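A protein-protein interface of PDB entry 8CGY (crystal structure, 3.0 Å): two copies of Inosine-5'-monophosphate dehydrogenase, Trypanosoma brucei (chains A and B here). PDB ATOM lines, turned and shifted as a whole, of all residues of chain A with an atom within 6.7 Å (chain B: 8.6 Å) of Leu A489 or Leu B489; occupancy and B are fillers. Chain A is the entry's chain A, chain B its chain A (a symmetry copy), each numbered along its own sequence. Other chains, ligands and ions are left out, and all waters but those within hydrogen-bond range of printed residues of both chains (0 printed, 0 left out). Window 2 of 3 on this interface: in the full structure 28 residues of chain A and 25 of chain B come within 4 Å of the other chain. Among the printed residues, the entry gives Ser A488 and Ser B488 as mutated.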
ATOM      1  N   ASP A  24       0.643 -12.481 -12.323  1.00  0.00           N
ATOM      2  CA  ASP A  24       1.325 -11.208 -12.519  1.00  0.00           C
ATOM      3  C   ASP A  24       2.821 -11.393 -12.764  1.00  0.00           C
ATOM      4  O   ASP A  24       3.430 -12.391 -12.365  1.00  0.00           O
ATOM      5  CB  ASP A  24       1.106 -10.294 -11.306  1.00  0.00           C
ATOM      6  CG  ASP A  24       1.491 -10.949  -9.989  1.00  0.00           C
ATOM      7  OD1 ASP A  24       1.729 -12.174  -9.969  1.00  0.00           O
ATOM      8  OD2 ASP A  24       1.556 -10.225  -8.971  1.00  0.00           O
ATOM      9  N   GLY A  25       3.402 -10.402 -13.437  1.00  0.00           N
ATOM     10  CA  GLY A  25       4.813 -10.455 -13.773  1.00  0.00           C
ATOM     11  C   GLY A  25       5.690 -10.318 -12.543  1.00  0.00           C
ATOM     12  O   GLY A  25       5.414  -9.535 -11.633  1.00  0.00           O
ATOM     13  N   ASP A  30      10.772 -11.807  -6.131  1.00  0.00           N
ATOM     14  CA  ASP A  30       9.456 -12.337  -5.791  1.00  0.00           C
ATOM     15  C   ASP A  30       9.478 -13.837  -5.494  1.00  0.00           C
ATOM     16  O   ASP A  30       8.498 -14.346  -4.938  1.00  0.00           O
ATOM     17  CB  ASP A  30       8.458 -12.042  -6.924  1.00  0.00           C
ATOM     18  CG  ASP A  30       7.921 -10.599  -6.907  1.00  0.00           C
ATOM     19  OD1 ASP A  30       7.262 -10.199  -5.925  1.00  0.00           O
ATOM     20  OD2 ASP A  30       8.150  -9.871  -7.896  1.00  0.00           O
ATOM     21  N   ARG A 486       7.135 -18.664  -4.141  1.00  0.00           N
ATOM     22  CA  ARG A 486       6.912 -17.227  -4.182  1.00  0.00           C
ATOM     23  C   ARG A 486       6.958 -16.677  -2.763  1.00  0.00           C
ATOM     24  O   ARG A 486       6.515 -17.332  -1.816  1.00  0.00           O
ATOM     25  CB  ARG A 486       5.573 -16.903  -4.836  1.00  0.00           C
ATOM     26  CG  ARG A 486       5.518 -15.524  -5.468  1.00  0.00           C
ATOM     27  CD  ARG A 486       4.087 -15.051  -5.573  1.00  0.00           C
ATOM     28  NE  ARG A 486       3.976 -13.624  -5.844  1.00  0.00           N
ATOM     29  CZ  ARG A 486       3.414 -13.119  -6.932  1.00  0.00           C
ATOM     30  NH1 ARG A 486       2.931 -13.898  -7.886  1.00  0.00           N
ATOM     31  NH2 ARG A 486       3.318 -11.799  -7.061  1.00  0.00           N
ATOM     32  N   ARG A 487       7.509 -15.480  -2.614  1.00  0.00           N
ATOM     33  CA  ARG A 487       7.701 -14.869  -1.307  1.00  0.00           C
ATOM     34  C   ARG A 487       6.776 -13.672  -1.165  1.00  0.00           C
ATOM     35  O   ARG A 487       6.755 -12.795  -2.035  1.00  0.00           O
ATOM     36  CB  ARG A 487       9.152 -14.427  -1.120  1.00  0.00           C
ATOM     37  CG  ARG A 487      10.162 -15.534  -1.322  1.00  0.00           C
ATOM     38  CD  ARG A 487      11.510 -15.114  -0.788  1.00  0.00           C
ATOM     39  NE  ARG A 487      12.138 -14.119  -1.647  1.00  0.00           N
ATOM     40  CZ  ARG A 487      13.132 -13.329  -1.268  1.00  0.00           C
ATOM     41  NH1 ARG A 487      13.608 -13.359  -0.035  1.00  0.00           N
ATOM     42  NH2 ARG A 487      13.660 -12.485  -2.147  1.00  0.00           N
ATOM     43  N   SER A 488       6.017 -13.629  -0.075  1.00  0.00           N
ATOM     44  CA  SER A 488       5.215 -12.445   0.174  1.00  0.00           C
ATOM     45  C   SER A 488       6.135 -11.235   0.311  1.00  0.00           C
ATOM     46  O   SER A 488       7.351 -11.361   0.485  1.00  0.00           O
ATOM     47  CB  SER A 488       4.357 -12.616   1.430  1.00  0.00           C
ATOM     48  OG  SER A 488       5.129 -12.466   2.608  1.00  0.00           O
ATOM     49  N   LEU A 489       5.548 -10.042   0.201  1.00  0.00           N
ATOM     50  CA  LEU A 489       6.353  -8.833   0.334  1.00  0.00           C
ATOM     51  C   LEU A 489       6.986  -8.752   1.714  1.00  0.00           C
ATOM     52  O   LEU A 489       8.154  -8.368   1.850  1.00  0.00           O
ATOM     53  CB  LEU A 489       5.510  -7.596   0.057  1.00  0.00           C
ATOM     54  CG  LEU A 489       5.307  -7.317  -1.429  1.00  0.00           C
ATOM     55  CD1 LEU A 489       4.943  -5.857  -1.638  1.00  0.00           C
ATOM     56  CD2 LEU A 489       6.553  -7.704  -2.224  1.00  0.00           C
ATOM     57  N   THR A 490       6.231  -9.109   2.750  1.00  0.00           N
ATOM     58  CA  THR A 490       6.799  -9.166   4.089  1.00  0.00           C
ATOM     59  C   THR A 490       7.980 -10.129   4.129  1.00  0.00           C
ATOM     60  O   THR A 490       9.047  -9.808   4.667  1.00  0.00           O
ATOM     61  CB  THR A 490       5.720  -9.584   5.087  1.00  0.00           C
ATOM     62  OG1 THR A 490       4.615  -8.677   4.994  1.00  0.00           O
ATOM     63  CG2 THR A 490       6.266  -9.571   6.503  1.00  0.00           C
ATOM     64  N   ALA A 491       7.813 -11.314   3.532  1.00  0.00           N
ATOM     65  CA  ALA A 491       8.895 -12.292   3.531  1.00  0.00           C
ATOM     66  C   ALA A 491      10.141 -11.755   2.838  1.00  0.00           C
ATOM     67  O   ALA A 491      11.256 -12.193   3.141  1.00  0.00           O
ATOM     68  CB  ALA A 491       8.429 -13.586   2.865  1.00  0.00           C
ATOM     69  N   GLN A 492       9.976 -10.817   1.902  1.00  0.00           N
ATOM     70  CA  GLN A 492      11.133 -10.224   1.242  1.00  0.00           C
ATOM     71  C   GLN A 492      11.845  -9.223   2.152  1.00  0.00           C
ATOM     72  O   GLN A 492      13.078  -9.137   2.132  1.00  0.00           O
ATOM     73  CB  GLN A 492      10.709  -9.558  -0.075  1.00  0.00           C
ATOM     74  CG  GLN A 492       9.868 -10.438  -1.011  1.00  0.00           C
ATOM     75  CD  GLN A 492       9.674  -9.818  -2.391  1.00  0.00           C
ATOM     76  OE1 GLN A 492      10.477  -8.997  -2.832  1.00  0.00           O
ATOM     77  NE2 GLN A 492       8.604 -10.210  -3.073  1.00  0.00           N
ATOM     78  N   SER A 493      11.086  -8.476   2.962  1.00  0.00           N
ATOM     79  CA  SER A 493      11.691  -7.520   3.889  1.00  0.00           C
ATOM     80  C   SER A 493      12.613  -8.206   4.886  1.00  0.00           C
ATOM     81  O   SER A 493      13.603  -7.612   5.328  1.00  0.00           O
ATOM     82  CB  SER A 493      10.605  -6.748   4.645  1.00  0.00           C
ATOM     83  OG  SER A 493       9.829  -5.934   3.782  1.00  0.00           O
ATOM     84  N   GLU A 494      12.294  -9.437   5.265  1.00  0.00           N
ATOM     85  CA  GLU A 494      13.061 -10.162   6.267  1.00  0.00           C
ATOM     86  C   GLU A 494      14.144 -11.008   5.607  1.00  0.00           C
ATOM     87  O   GLU A 494      14.367 -12.159   5.980  1.00  0.00           O
ATOM     88  CB  GLU A 494      12.137 -11.033   7.113  1.00  0.00           C
ATOM     89  N   LEU B  26      -6.864  -0.909  -9.947  1.00  0.00           N
ATOM     90  CA  LEU B  26      -5.479  -0.737 -10.346  1.00  0.00           C
ATOM     91  C   LEU B  26      -5.153   0.723 -10.607  1.00  0.00           C
ATOM     92  O   LEU B  26      -5.977   1.475 -11.139  1.00  0.00           O
ATOM     93  CB  LEU B  26      -5.168  -1.540 -11.597  1.00  0.00           C
ATOM     94  CG  LEU B  26      -5.146  -3.058 -11.465  1.00  0.00           C
ATOM     95  CD1 LEU B  26      -4.591  -3.602 -12.752  1.00  0.00           C
ATOM     96  CD2 LEU B  26      -4.287  -3.465 -10.289  1.00  0.00           C
ATOM     97  N   ASN B  29       0.551   2.258 -12.488  1.00  0.00           N
ATOM     98  CA  ASN B  29       1.827   1.597 -12.261  1.00  0.00           C
ATOM     99  C   ASN B  29       1.692   0.103 -12.005  1.00  0.00           C
ATOM    100  O   ASN B  29       2.712  -0.596 -11.992  1.00  0.00           O
ATOM    101  CB  ASN B  29       2.554   2.263 -11.099  1.00  0.00           C
ATOM    102  CG  ASN B  29       2.928   3.686 -11.405  1.00  0.00           C
ATOM    103  OD1 ASN B  29       2.190   4.616 -11.087  1.00  0.00           O
ATOM    104  ND2 ASN B  29       4.066   3.868 -12.064  1.00  0.00           N
ATOM    105  N   ASP B  30       0.468  -0.399 -11.804  1.00  0.00           N
ATOM    106  CA  ASP B  30       0.264  -1.820 -11.548  1.00  0.00           C
ATOM    107  C   ASP B  30       0.426  -2.679 -12.802  1.00  0.00           C
ATOM    108  O   ASP B  30       0.547  -3.903 -12.672  1.00  0.00           O
ATOM    109  CB  ASP B  30      -1.125  -2.052 -10.930  1.00  0.00           C
ATOM    110  CG  ASP B  30      -1.186  -1.735  -9.424  1.00  0.00           C
ATOM    111  OD1 ASP B  30      -0.481  -2.389  -8.628  1.00  0.00           O
ATOM    112  OD2 ASP B  30      -1.963  -0.835  -9.040  1.00  0.00           O
ATOM    113  N   ARG B 486       0.443  -7.473 -15.567  1.00  0.00           N
ATOM    114  CA  ARG B 486       0.441  -6.893 -14.233  1.00  0.00           C
ATOM    115  C   ARG B 486       1.820  -7.070 -13.613  1.00  0.00           C
ATOM    116  O   ARG B 486       2.487  -8.085 -13.831  1.00  0.00           O
ATOM    117  CB  ARG B 486      -0.625  -7.545 -13.358  1.00  0.00           C
ATOM    118  CG  ARG B 486      -1.120  -6.656 -12.231  1.00  0.00           C
ATOM    119  CD  ARG B 486      -1.697  -7.495 -11.115  1.00  0.00           C
ATOM    120  NE  ARG B 486      -1.873  -6.753  -9.875  1.00  0.00           N
ATOM    121  CZ  ARG B 486      -3.046  -6.551  -9.293  1.00  0.00           C
ATOM    122  NH1 ARG B 486      -4.169  -6.996  -9.831  1.00  0.00           N
ATOM    123  NH2 ARG B 486      -3.093  -5.901  -8.134  1.00  0.00           N
ATOM    124  N   ARG B 487       2.255  -6.075 -12.852  1.00  0.00           N
ATOM    125  CA  ARG B 487       3.588  -6.067 -12.268  1.00  0.00           C
ATOM    126  C   ARG B 487       3.482  -6.223 -10.760  1.00  0.00           C
ATOM    127  O   ARG B 487       2.737  -5.484 -10.109  1.00  0.00           O
ATOM    128  CB  ARG B 487       4.323  -4.769 -12.603  1.00  0.00           C
ATOM    129  CG  ARG B 487       4.411  -4.479 -14.084  1.00  0.00           C
ATOM    130  CD  ARG B 487       5.429  -3.394 -14.343  1.00  0.00           C
ATOM    131  NE  ARG B 487       4.939  -2.090 -13.918  1.00  0.00           N
ATOM    132  CZ  ARG B 487       5.715  -1.037 -13.701  1.00  0.00           C
ATOM    133  NH1 ARG B 487       7.030  -1.112 -13.816  1.00  0.00           N
ATOM    134  NH2 ARG B 487       5.158   0.118 -13.356  1.00  0.00           N
ATOM    135  N   SER B 488       4.223  -7.177 -10.205  1.00  0.00           N
ATOM    136  CA  SER B 488       4.260  -7.281  -8.757  1.00  0.00           C
ATOM    137  C   SER B 488       4.818  -5.986  -8.174  1.00  0.00           C
ATOM    138  O   SER B 488       5.410  -5.161  -8.877  1.00  0.00           O
ATOM    139  CB  SER B 488       5.102  -8.480  -8.314  1.00  0.00           C
ATOM    140  OG  SER B 488       6.487  -8.211  -8.433  1.00  0.00           O
ATOM    141  N   LEU B 489       4.600  -5.792  -6.872  1.00  0.00           N
ATOM    142  CA  LEU B 489       5.114  -4.586  -6.233  1.00  0.00           C
ATOM    143  C   LEU B 489       6.631  -4.532  -6.314  1.00  0.00           C
ATOM    144  O   LEU B 489       7.211  -3.468  -6.562  1.00  0.00           O
ATOM    145  CB  LEU B 489       4.652  -4.512  -4.783  1.00  0.00           C
ATOM    146  CG  LEU B 489       3.221  -4.006  -4.625  1.00  0.00           C
ATOM    147  CD1 LEU B 489       3.014  -3.467  -3.221  1.00  0.00           C
ATOM    148  CD2 LEU B 489       2.902  -2.953  -5.685  1.00  0.00           C
ATOM    149  N   THR B 490       7.290  -5.670  -6.109  1.00  0.00           N
ATOM    150  CA  THR B 490       8.736  -5.723  -6.281  1.00  0.00           C
ATOM    151  C   THR B 490       9.122  -5.309  -7.697  1.00  0.00           C
ATOM    152  O   THR B 490      10.033  -4.497  -7.897  1.00  0.00           O
ATOM    153  CB  THR B 490       9.238  -7.132  -5.968  1.00  0.00           C
ATOM    154  OG1 THR B 490       8.824  -7.497  -4.645  1.00  0.00           O
ATOM    155  CG2 THR B 490      10.752  -7.194  -6.059  1.00  0.00           C
ATOM    156  N   ALA B 491       8.411  -5.841  -8.696  1.00  0.00           N
ATOM    157  CA  ALA B 491       8.722  -5.497 -10.079  1.00  0.00           C
ATOM    158  C   ALA B 491       8.572  -4.004 -10.338  1.00  0.00           C
ATOM    159  O   ALA B 491       9.222  -3.464 -11.239  1.00  0.00           O
ATOM    160  CB  ALA B 491       7.830  -6.296 -11.029  1.00  0.00           C
ATOM    161  N   GLN B 492       7.720  -3.322  -9.569  1.00  0.00           N
ATOM    162  CA  GLN B 492       7.574  -1.881  -9.730  1.00  0.00           C
ATOM    163  C   GLN B 492       8.757  -1.127  -9.125  1.00  0.00           C
ATOM    164  O   GLN B 492       9.193  -0.110  -9.679  1.00  0.00           O
ATOM    165  CB  GLN B 492       6.252  -1.408  -9.109  1.00  0.00           C
ATOM    166  CG  GLN B 492       5.006  -2.192  -9.549  1.00  0.00           C
ATOM    167  CD  GLN B 492       3.705  -1.541  -9.091  1.00  0.00           C
ATOM    168  OE1 GLN B 492       3.653  -0.336  -8.852  1.00  0.00           O
ATOM    169  NE2 GLN B 492       2.653  -2.343  -8.967  1.00  0.00           N
ATOM    170  N   SER B 493       9.296  -1.619  -8.003  1.00  0.00           N
ATOM    171  CA  SER B 493      10.453  -0.977  -7.380  1.00  0.00           C
ATOM    172  C   SER B 493      11.657  -0.958  -8.310  1.00  0.00           C
ATOM    173  O   SER B 493      12.474  -0.032  -8.251  1.00  0.00           O
ATOM    174  CB  SER B 493      10.825  -1.694  -6.079  1.00  0.00           C
ATOM    175  OG  SER B 493       9.809  -1.580  -5.097  1.00  0.00           O
ATOM    176  N   GLU B 494      11.794  -1.975  -9.152  1.00  0.00           N
ATOM    177  CA  GLU B 494      12.944  -2.099 -10.037  1.00  0.00           C
ATOM    178  C   GLU B 494      12.654  -1.456 -11.389  1.00  0.00           C
ATOM    179  O   GLU B 494      12.988  -2.005 -12.437  1.00  0.00           O
ATOM    180  CB  GLU B 494      13.323  -3.566 -10.207  1.00  0.00           C
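The backbone carbonyl oxygen (O) of Arg B486 sits at hydrogen-bond distance from the backbone NH (N) of Gly A25 (2.5 Å). The backbone carbonyl oxygen (O) of Gly A25 is in hydrogen-bond range of the backbone NH (N) of Ser B488 (3.0 Å). The side-chain carboxylate (OD2) of Asp A30 is in hydrogen-bond range of the side-chain hydroxyl (OG) of Ser B488 (2.4 Å). The side-chain carboxylate of Asp A30 sits at hydrogen-bond distance from the side-chain hydroxyl of Thr B490 (3.4 Å). OE1 of Gln A492 sits at hydrogen-bond distance from OG1 of Thr B490.
The backbone NH (N) of Arg B487 is in hydrogen-bond range of the backbone carbonyl oxygen (O) of Asp B30, 2.8 Å away. The backbone carbonyl oxygen of Asp A30 is in hydrogen-bond range of the backbone NH of Arg A487. NE2 of Gln A492 sits at hydrogen-bond distance from O of Arg A487. The guanidinium group (NH1) of Arg A486 lies within salt-bridge range of the side-chain carboxylate (OD1) of Asp A24, 3.0 Å away. NH2 of Arg B487 lies within hydrogen-bond range of O of Asn B29 (2.9 Å). The backbone carbonyl oxygen of Arg B487 lies within hydrogen-bond range of the side-chain amide nitrogen of Gln B492 (3.3 Å).
Among the printed residues, merely in contact across the chains: Leu A489 with Thr B490, Leu A489 with Leu B489, Asp A24 with Arg B486, Gly A25 with Arg B487 and Arg A486 with Ser B488.
Printed residues of chain B within 4 Å of Gly A25: Arg B486, Arg B487 and Ser B488. Printed residues of chain B within 4 Å of Asp A30: Ser B488 (2.4 Å) and Thr B490 (3.4 Å). Printed residues of chain B within 4 Å of Arg A486: Ser B488 (3.97 Å). No residue of chain B comes within 4 Å of Ser A488. Leu A489 touches just these residues of chain B: Leu B489 (3.4 Å) and Thr B490 (3.3 Å). Printed residues of chain B within 4 Å of Gln A492: Thr B490. Printed residues of chain A within 4 Å of Arg B487: Gly A25. The nearest printed residue of chain B that does not touch Asp A24 is Ser B488 (4.003 Å).
Hydrophobic or aromatic side chains of chain B that line the printed part of chain A: Leu B489. Hydrophobic or aromatic side chains of chain A within 4 Å of the printed part of chain B: Leu A489.
Asp A30 touches Ser B488, but with the chains exchanged Ser A488 does not touch Asp B30 (14.2 Å). Asp A30 touches Thr B490, but with the chains exchanged Thr A490 does not touch Asp B30 (14.8 Å). Arg A486 touches Ser B488, but with the chains exchanged Ser A488 does not touch Arg B486 (13.4 Å). Leu A489 touches its own counterpart, Leu B489. Positions printed for both chains: 30, 486, 487, 488, 489, 490, 491, 492, 493 and 494. Of the 10 pairs that touch across the chains among the printed residues, 1 has its exchanged pair printed and touching as well.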
